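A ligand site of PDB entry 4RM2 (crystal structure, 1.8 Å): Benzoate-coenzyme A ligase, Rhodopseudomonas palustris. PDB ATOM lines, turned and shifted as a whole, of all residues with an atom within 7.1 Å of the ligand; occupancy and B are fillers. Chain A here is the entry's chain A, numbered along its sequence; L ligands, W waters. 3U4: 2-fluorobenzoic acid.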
ATOM      1  N   PHE A 221       8.330  -9.296 -15.642  1.00  0.00           N
ATOM      2  CA  PHE A 221       9.282 -10.368 -15.587  1.00  0.00           C
ATOM      3  C   PHE A 221       8.535 -11.686 -15.728  1.00  0.00           C
ATOM      4  O   PHE A 221       7.540 -11.877 -15.052  1.00  0.00           O
ATOM      5  CB  PHE A 221      10.006 -10.411 -14.278  1.00  0.00           C
ATOM      6  CG  PHE A 221      11.028  -9.297 -14.099  1.00  0.00           C
ATOM      7  CD1 PHE A 221      12.223  -9.288 -14.826  1.00  0.00           C
ATOM      8  CD2 PHE A 221      10.812  -8.340 -13.159  1.00  0.00           C
ATOM      9  CE1 PHE A 221      13.175  -8.264 -14.614  1.00  0.00           C
ATOM     10  CE2 PHE A 221      11.757  -7.351 -12.936  1.00  0.00           C
ATOM     11  CZ  PHE A 221      12.886  -7.303 -13.657  1.00  0.00           C
ATOM     12  N   ALA A 222       9.046 -12.588 -16.551  1.00  0.00           N
ATOM     13  CA  ALA A 222       8.447 -13.928 -16.561  1.00  0.00           C
ATOM     14  C   ALA A 222       8.275 -14.472 -15.151  1.00  0.00           C
ATOM     15  O   ALA A 222       7.246 -15.053 -14.788  1.00  0.00           O
ATOM     16  CB  ALA A 222       9.312 -14.848 -17.423  1.00  0.00           C
ATOM     17  N   TYR A 223       9.321 -14.338 -14.322  1.00  0.00           N
ATOM     18  CA  TYR A 223       9.267 -14.874 -12.938  1.00  0.00           C
ATOM     19  C   TYR A 223       8.047 -14.273 -12.239  1.00  0.00           C
ATOM     20  O   TYR A 223       7.217 -15.022 -11.691  1.00  0.00           O
ATOM     21  CB  TYR A 223      10.558 -14.526 -12.201  1.00  0.00           C
ATOM     22  CG  TYR A 223      10.669 -14.943 -10.763  1.00  0.00           C
ATOM     23  CD1 TYR A 223      10.398 -16.264 -10.384  1.00  0.00           C
ATOM     24  CD2 TYR A 223      11.225 -14.068  -9.808  1.00  0.00           C
ATOM     25  CE1 TYR A 223      10.514 -16.661  -9.077  1.00  0.00           C
ATOM     26  CE2 TYR A 223      11.365 -14.461  -8.499  1.00  0.00           C
ATOM     27  CZ  TYR A 223      11.030 -15.760  -8.138  1.00  0.00           C
ATOM     28  OH  TYR A 223      11.201 -16.148  -6.849  1.00  0.00           O
ATOM     29  N   GLY A 224       7.910 -12.945 -12.268  1.00  0.00           N
ATOM     30  CA  GLY A 224       6.791 -12.258 -11.601  1.00  0.00           C
ATOM     31  C   GLY A 224       5.412 -12.486 -12.191  1.00  0.00           C
ATOM     32  O   GLY A 224       4.400 -12.630 -11.423  1.00  0.00           O
ATOM     33  N   ASN A 227       4.494 -15.703 -10.610  1.00  0.00           N
ATOM     34  CA  ASN A 227       4.350 -15.554  -9.155  1.00  0.00           C
ATOM     35  C   ASN A 227       3.064 -14.854  -8.756  1.00  0.00           C
ATOM     36  O   ASN A 227       2.473 -15.194  -7.718  1.00  0.00           O
ATOM     37  CB  ASN A 227       5.553 -14.740  -8.584  1.00  0.00           C
ATOM     38  CG  ASN A 227       6.920 -15.374  -8.838  1.00  0.00           C
ATOM     39  OD1 ASN A 227       7.050 -16.561  -9.264  1.00  0.00           O
ATOM     40  ND2 ASN A 227       7.974 -14.547  -8.701  1.00  0.00           N
ATOM     41  N   SER A 296      12.925 -17.842  -4.534  1.00  0.00           N
ATOM     42  CA  SER A 296      13.940 -16.970  -5.151  1.00  0.00           C
ATOM     43  C   SER A 296      14.337 -17.394  -6.522  1.00  0.00           C
ATOM     44  O   SER A 296      14.445 -18.535  -6.819  1.00  0.00           O
ATOM     45  CB  SER A 296      15.205 -16.732  -4.292  1.00  0.00           C
ATOM     46  OG  SER A 296      16.156 -17.811  -4.296  1.00  0.00           O
ATOM     47  N   ALA A 297      14.531 -16.396  -7.364  1.00  0.00           N
ATOM     48  CA  ALA A 297      15.119 -16.558  -8.659  1.00  0.00           C
ATOM     49  C   ALA A 297      15.721 -15.248  -9.072  1.00  0.00           C
ATOM     50  O   ALA A 297      15.437 -14.235  -8.505  1.00  0.00           O
ATOM     51  CB  ALA A 297      14.035 -16.941  -9.647  1.00  0.00           C
ATOM     52  N   GLY A 298      16.488 -15.283 -10.140  1.00  0.00           N
ATOM     53  CA  GLY A 298      17.015 -14.068 -10.755  1.00  0.00           C
ATOM     54  C   GLY A 298      18.552 -14.006 -10.725  1.00  0.00           C
ATOM     55  O   GLY A 298      19.150 -13.198 -11.395  1.00  0.00           O
ATOM     56  N   GLU A 299      19.154 -14.879  -9.974  1.00  0.00           N
ATOM     57  CA  GLU A 299      20.613 -15.123  -9.898  1.00  0.00           C
ATOM     58  C   GLU A 299      20.772 -16.322  -8.932  1.00  0.00           C
ATOM     59  O   GLU A 299      19.818 -16.689  -8.254  1.00  0.00           O
ATOM     60  CB  GLU A 299      21.357 -13.894  -9.365  1.00  0.00           C
ATOM     61  CG  GLU A 299      20.853 -13.401  -7.975  1.00  0.00           C
ATOM     62  CD  GLU A 299      21.257 -12.007  -7.626  1.00  0.00           C
ATOM     63  OE1 GLU A 299      22.447 -11.685  -8.049  1.00  0.00           O
ATOM     64  OE2 GLU A 299      20.445 -11.268  -7.000  1.00  0.00           O
ATOM     65  N   ASP A 319      15.179 -21.764  -3.977  1.00  0.00           N
ATOM     66  CA  ASP A 319      15.859 -21.184  -5.197  1.00  0.00           C
ATOM     67  C   ASP A 319      15.552 -22.108  -6.378  1.00  0.00           C
ATOM     68  O   ASP A 319      15.710 -23.346  -6.261  1.00  0.00           O
ATOM     69  CB  ASP A 319      17.353 -21.117  -4.878  1.00  0.00           C
ATOM     70  CG  ASP A 319      18.290 -20.869  -6.068  1.00  0.00           C
ATOM     71  OD1 ASP A 319      17.923 -20.315  -7.125  1.00  0.00           O
ATOM     72  OD2 ASP A 319      19.513 -21.148  -5.913  1.00  0.00           O
ATOM     73  N   GLY A 320      15.154 -21.537  -7.522  1.00  0.00           N
ATOM     74  CA  GLY A 320      14.978 -22.305  -8.761  1.00  0.00           C
ATOM     75  C   GLY A 320      15.388 -21.359  -9.902  1.00  0.00           C
ATOM     76  O   GLY A 320      15.666 -20.182  -9.696  1.00  0.00           O
ATOM     77  N   ILE A 321      15.585 -21.947 -11.068  1.00  0.00           N
ATOM     78  CA  ILE A 321      15.963 -21.243 -12.253  1.00  0.00           C
ATOM     79  C   ILE A 321      14.945 -21.494 -13.339  1.00  0.00           C
ATOM     80  O   ILE A 321      14.504 -22.622 -13.596  1.00  0.00           O
ATOM     81  CB  ILE A 321      17.408 -21.574 -12.743  1.00  0.00           C
ATOM     82  CG1 ILE A 321      17.792 -20.619 -13.892  1.00  0.00           C
ATOM     83  CG2 ILE A 321      17.592 -23.054 -13.056  1.00  0.00           C
ATOM     84  CD1 ILE A 321      19.276 -20.543 -14.148  1.00  0.00           C
ATOM     85  N   GLY A 322      14.580 -20.389 -13.971  1.00  0.00           N
ATOM     86  CA  GLY A 322      13.765 -20.362 -15.165  1.00  0.00           C
ATOM     87  C   GLY A 322      14.392 -19.498 -16.222  1.00  0.00           C
ATOM     88  O   GLY A 322      15.564 -19.048 -16.080  1.00  0.00           O
ATOM     89  N   SER A 323      13.662 -19.192 -17.277  1.00  0.00           N
ATOM     90  CA  SER A 323      14.122 -18.208 -18.256  1.00  0.00           C
ATOM     91  C   SER A 323      12.921 -17.618 -18.926  1.00  0.00           C
ATOM     92  O   SER A 323      11.843 -18.191 -18.866  1.00  0.00           O
ATOM     93  CB  SER A 323      14.991 -18.856 -19.350  1.00  0.00           C
ATOM     94  OG  SER A 323      14.260 -19.793 -20.120  1.00  0.00           O
ATOM     95  N   THR A 324      13.108 -16.445 -19.565  1.00  0.00           N
ATOM     96  CA  THR A 324      12.026 -15.865 -20.367  1.00  0.00           C
ATOM     97  C   THR A 324      11.538 -16.847 -21.390  1.00  0.00           C
ATOM     98  O   THR A 324      10.354 -17.058 -21.582  1.00  0.00           O
ATOM     99  CB  THR A 324      12.546 -14.593 -21.053  1.00  0.00           C
ATOM    100  OG1 THR A 324      13.242 -13.757 -20.091  1.00  0.00           O
ATOM    101  CG2 THR A 324      11.402 -13.798 -21.706  1.00  0.00           C
ATOM    102  N   GLU A 325      12.487 -17.532 -22.024  1.00  0.00           N
ATOM    103  CA  GLU A 325      12.138 -18.501 -23.085  1.00  0.00           C
ATOM    104  C   GLU A 325      11.338 -19.722 -22.606  1.00  0.00           C
ATOM    105  O   GLU A 325      10.483 -20.253 -23.324  1.00  0.00           O
ATOM    106  CB  GLU A 325      13.443 -18.943 -23.758  1.00  0.00           C
ATOM    107  CG  GLU A 325      14.057 -17.879 -24.664  1.00  0.00           C
ATOM    108  CD  GLU A 325      15.033 -16.970 -23.918  1.00  0.00           C
ATOM    109  OE1 GLU A 325      15.159 -17.016 -22.634  1.00  0.00           O
ATOM    110  OE2 GLU A 325      15.612 -16.059 -24.590  1.00  0.00           O
ATOM    111  N   MET A 326      11.659 -20.243 -21.401  1.00  0.00           N
ATOM    112  CA  MET A 326      10.898 -21.327 -20.815  1.00  0.00           C
ATOM    113  C   MET A 326       9.711 -20.881 -19.956  1.00  0.00           C
ATOM    114  O   MET A 326       8.931 -21.726 -19.478  1.00  0.00           O
ATOM    115  CB  MET A 326      11.830 -22.251 -19.979  1.00  0.00           C
ATOM    116  CG  MET A 326      12.907 -22.951 -20.784  1.00  0.00           C
ATOM    117  SD  MET A 326      12.217 -23.942 -22.136  1.00  0.00           S
ATOM    118  CE  MET A 326      11.101 -25.026 -21.337  1.00  0.00           C
ATOM    119  N   LEU A 327       9.524 -19.550 -19.833  1.00  0.00           N
ATOM    120  CA  LEU A 327       8.413 -18.935 -19.121  1.00  0.00           C
ATOM    121  C   LEU A 327       8.487 -18.967 -17.640  1.00  0.00           C
ATOM    122  O   LEU A 327       8.145 -17.971 -16.996  1.00  0.00           O
ATOM    123  CB  LEU A 327       7.086 -19.363 -19.613  1.00  0.00           C
ATOM    124  CG  LEU A 327       5.906 -18.477 -19.145  1.00  0.00           C
ATOM    125  CD1 LEU A 327       5.971 -16.987 -19.444  1.00  0.00           C
ATOM    126  CD2 LEU A 327       4.652 -19.112 -19.706  1.00  0.00           C
ATOM    127  N   HIS A 328       8.842 -20.101 -17.061  1.00  0.00           N
ATOM    128  CA  HIS A 328       9.090 -20.162 -15.602  1.00  0.00           C
ATOM    129  C   HIS A 328      10.111 -21.275 -15.217  1.00  0.00           C
ATOM    130  O   HIS A 328      10.854 -21.727 -16.049  1.00  0.00           O
ATOM    131  CB  HIS A 328       7.802 -20.226 -14.803  1.00  0.00           C
ATOM    132  CG  HIS A 328       7.829 -19.458 -13.508  1.00  0.00           C
ATOM    133  ND1 HIS A 328       8.287 -20.008 -12.331  1.00  0.00           N
ATOM    134  CD2 HIS A 328       7.335 -18.234 -13.169  1.00  0.00           C
ATOM    135  CE1 HIS A 328       8.196 -19.135 -11.360  1.00  0.00           C
ATOM    136  NE2 HIS A 328       7.607 -18.056 -11.834  1.00  0.00           N
ATOM    137  N   ILE A 329      10.162 -21.661 -13.937  1.00  0.00           N
ATOM    138  CA  ILE A 329      11.213 -22.419 -13.375  1.00  0.00           C
ATOM    139  C   ILE A 329      11.093 -23.882 -13.850  1.00  0.00           C
ATOM    140  O   ILE A 329      10.050 -24.505 -13.754  1.00  0.00           O
ATOM    141  CB  ILE A 329      11.166 -22.278 -11.833  1.00  0.00           C
ATOM    142  CG1 ILE A 329      11.648 -20.843 -11.467  1.00  0.00           C
ATOM    143  CG2 ILE A 329      12.047 -23.324 -11.179  1.00  0.00           C
ATOM    144  CD1 ILE A 329      11.481 -20.402 -10.014  1.00  0.00           C
ATOM    145  N   PHE A 330      12.208 -24.408 -14.308  1.00  0.00           N
ATOM    146  CA  PHE A 330      12.315 -25.787 -14.750  1.00  0.00           C
ATOM    147  C   PHE A 330      13.308 -26.651 -13.919  1.00  0.00           C
ATOM    148  O   PHE A 330      13.375 -27.889 -14.132  1.00  0.00           O
ATOM    149  CB  PHE A 330      12.699 -25.798 -16.233  1.00  0.00           C
ATOM    150  CG  PHE A 330      13.864 -24.911 -16.544  1.00  0.00           C
ATOM    151  CD1 PHE A 330      15.138 -25.302 -16.161  1.00  0.00           C
ATOM    152  CD2 PHE A 330      13.710 -23.696 -17.186  1.00  0.00           C
ATOM    153  CE1 PHE A 330      16.245 -24.502 -16.458  1.00  0.00           C
ATOM    154  CE2 PHE A 330      14.815 -22.886 -17.437  1.00  0.00           C
ATOM    155  CZ  PHE A 330      16.097 -23.294 -17.103  1.00  0.00           C
ATOM    156  N   LYS A 422      24.105 -11.507 -14.575  1.00  0.00           N
ATOM    157  CA  LYS A 422      22.752 -11.465 -14.017  1.00  0.00           C
ATOM    158  C   LYS A 422      22.818 -10.735 -12.714  1.00  0.00           C
ATOM    159  O   LYS A 422      23.407 -11.222 -11.785  1.00  0.00           O
ATOM    160  CB  LYS A 422      22.210 -12.890 -13.869  1.00  0.00           C
ATOM    161  CG  LYS A 422      20.885 -13.034 -14.598  1.00  0.00           C
ATOM    162  CD  LYS A 422      20.157 -14.337 -14.302  1.00  0.00           C
ATOM    163  CE  LYS A 422      18.635 -14.147 -14.437  1.00  0.00           C
ATOM    164  NZ  LYS A 422      18.037 -15.539 -14.323  1.00  0.00           N
ATOM    165  N   GLY A 425      18.265 -10.339 -11.186  1.00  0.00           N
ATOM    166  CA  GLY A 425      17.100 -10.638 -11.981  1.00  0.00           C
ATOM    167  C   GLY A 425      17.069  -9.991 -13.344  1.00  0.00           C
ATOM    168  O   GLY A 425      16.176 -10.319 -14.178  1.00  0.00           O
ATOM    169  N   ILE A 426      18.036  -9.100 -13.610  1.00  0.00           N
ATOM    170  CA  ILE A 426      18.066  -8.389 -14.868  1.00  0.00           C
ATOM    171  C   ILE A 426      19.420  -8.748 -15.400  1.00  0.00           C
ATOM    172  O   ILE A 426      20.421  -8.621 -14.695  1.00  0.00           O
ATOM    173  CB  ILE A 426      17.842  -6.871 -14.723  1.00  0.00           C
ATOM    174  CG1 ILE A 426      16.348  -6.588 -14.602  1.00  0.00           C
ATOM    175  CG2 ILE A 426      18.283  -6.120 -15.988  1.00  0.00           C
ATOM    176  CD1 ILE A 426      16.026  -5.118 -14.384  1.00  0.00           C
ATOM    177  N   TYR A 427      19.361  -9.290 -16.589  1.00  0.00           N
ATOM    178  CA  TYR A 427      20.517  -9.477 -17.358  1.00  0.00           C
ATOM    179  C   TYR A 427      21.066  -8.105 -17.728  1.00  0.00           C
ATOM    180  O   TYR A 427      20.294  -7.194 -18.112  1.00  0.00           O
ATOM    181  CB  TYR A 427      20.134 -10.278 -18.584  1.00  0.00           C
ATOM    182  CG  TYR A 427      20.119 -11.736 -18.342  1.00  0.00           C
ATOM    183  CD1 TYR A 427      21.299 -12.455 -18.206  1.00  0.00           C
ATOM    184  CD2 TYR A 427      18.922 -12.439 -18.318  1.00  0.00           C
ATOM    185  CE1 TYR A 427      21.296 -13.835 -18.022  1.00  0.00           C
ATOM    186  CE2 TYR A 427      18.915 -13.824 -18.126  1.00  0.00           C
ATOM    187  CZ  TYR A 427      20.102 -14.515 -17.981  1.00  0.00           C
ATOM    188  OH  TYR A 427      20.096 -15.889 -17.780  1.00  0.00           O
HETATM  189  C1  3U4 L   1      14.976 -16.823 -13.320  1.00  0.00           C
HETATM  190  C2  3U4 L   1      13.622 -16.959 -13.939  1.00  0.00           C
HETATM  191  C3  3U4 L   1      12.656 -17.613 -13.206  1.00  0.00           C
HETATM  192  C4  3U4 L   1      11.408 -17.667 -13.829  1.00  0.00           C
HETATM  193  C5  3U4 L   1      11.178 -17.122 -15.103  1.00  0.00           C
HETATM  194  C6  3U4 L   1      12.153 -16.450 -15.791  1.00  0.00           C
HETATM  195  C7  3U4 L   1      13.389 -16.380 -15.163  1.00  0.00           C
HETATM  196  O8  3U4 L   1      15.517 -15.672 -13.303  1.00  0.00           O
HETATM  197  O9  3U4 L   1      15.487 -17.911 -12.880  1.00  0.00           O
HETATM  198  F10 3U4 L   1      14.348 -15.730 -15.822  1.00  0.00           F
HETATM  199  O   HOH W   1      17.199 -16.914 -16.717  1.00  0.00           O
HETATM  200  O   HOH W   2      15.688 -15.235 -18.687  1.00  0.00           O
HETATM  201  O   HOH W   3      17.329 -18.002 -10.971  1.00  0.00           O
HETATM  202  O   HOH W   4      15.218 -13.034 -17.710  1.00  0.00           O
HETATM  203  O   HOH W   5      11.862 -13.198 -15.088  1.00  0.00           O
HETATM  204  O   HOH W   6      14.147 -13.409 -13.540  1.00  0.00           O
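Water W3 lies within hydrogen-bond range of O9 of the ligand (2.7 Å), N of Gly 298 (3.0 Å) and O of Gly 320 (3.0 Å).
Water W1 lies within hydrogen-bond range of O of Gly 322 (2.8 Å), NZ of Lys 422 (2.9 Å) and OH of Tyr 427 (3.3 Å).
Merely in contact with the ligand: Ala 222, Tyr 223, Ala 297, Gly 320, Ile 321, Ser 323, Thr 324, Leu 327, His 328 and Ile 329.
Of the 25 residues printed, 13 come within 4 Å of the ligand.
N of Gly 298 is in hydrogen-bond range of O8 of the ligand.
NZ of Lys 422 lies within salt-bridge range of O8 of the ligand.
The backbone NH (N) of Gly 322 is in hydrogen-bond range of an oxygen (O9) of the ligand.
The side-chain hydroxyl of Tyr 223 sits close to the backbone NH of Ser 296 (3.3 Å).
The side-chain hydroxyl (OG) of Ser 323 sits close to the backbone NH (N) of Glu 325.
O of Gly 298 is in hydrogen-bond range of N of Gly 425.
The side-chain hydroxyl (OH) of Tyr 223 is in hydrogen-bond range of the backbone NH (N) of Ala 297, 3.4 Å away.
The backbone NH of Gly 320 sits at hydrogen-bond distance from the backbone carbonyl oxygen of Ser 296, at 3.2 Å.
The backbone carbonyl oxygen (O) of Tyr 223 lies close to the side-chain amide oxygen (OD1) of Asn 227 (2.9 Å).
O of Tyr 223 is in hydrogen-bond range of NE2 of His 328, at 3.1 Å.
The backbone NH of Phe 330 is in hydrogen-bond range of the backbone carbonyl oxygen of Ile 321.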
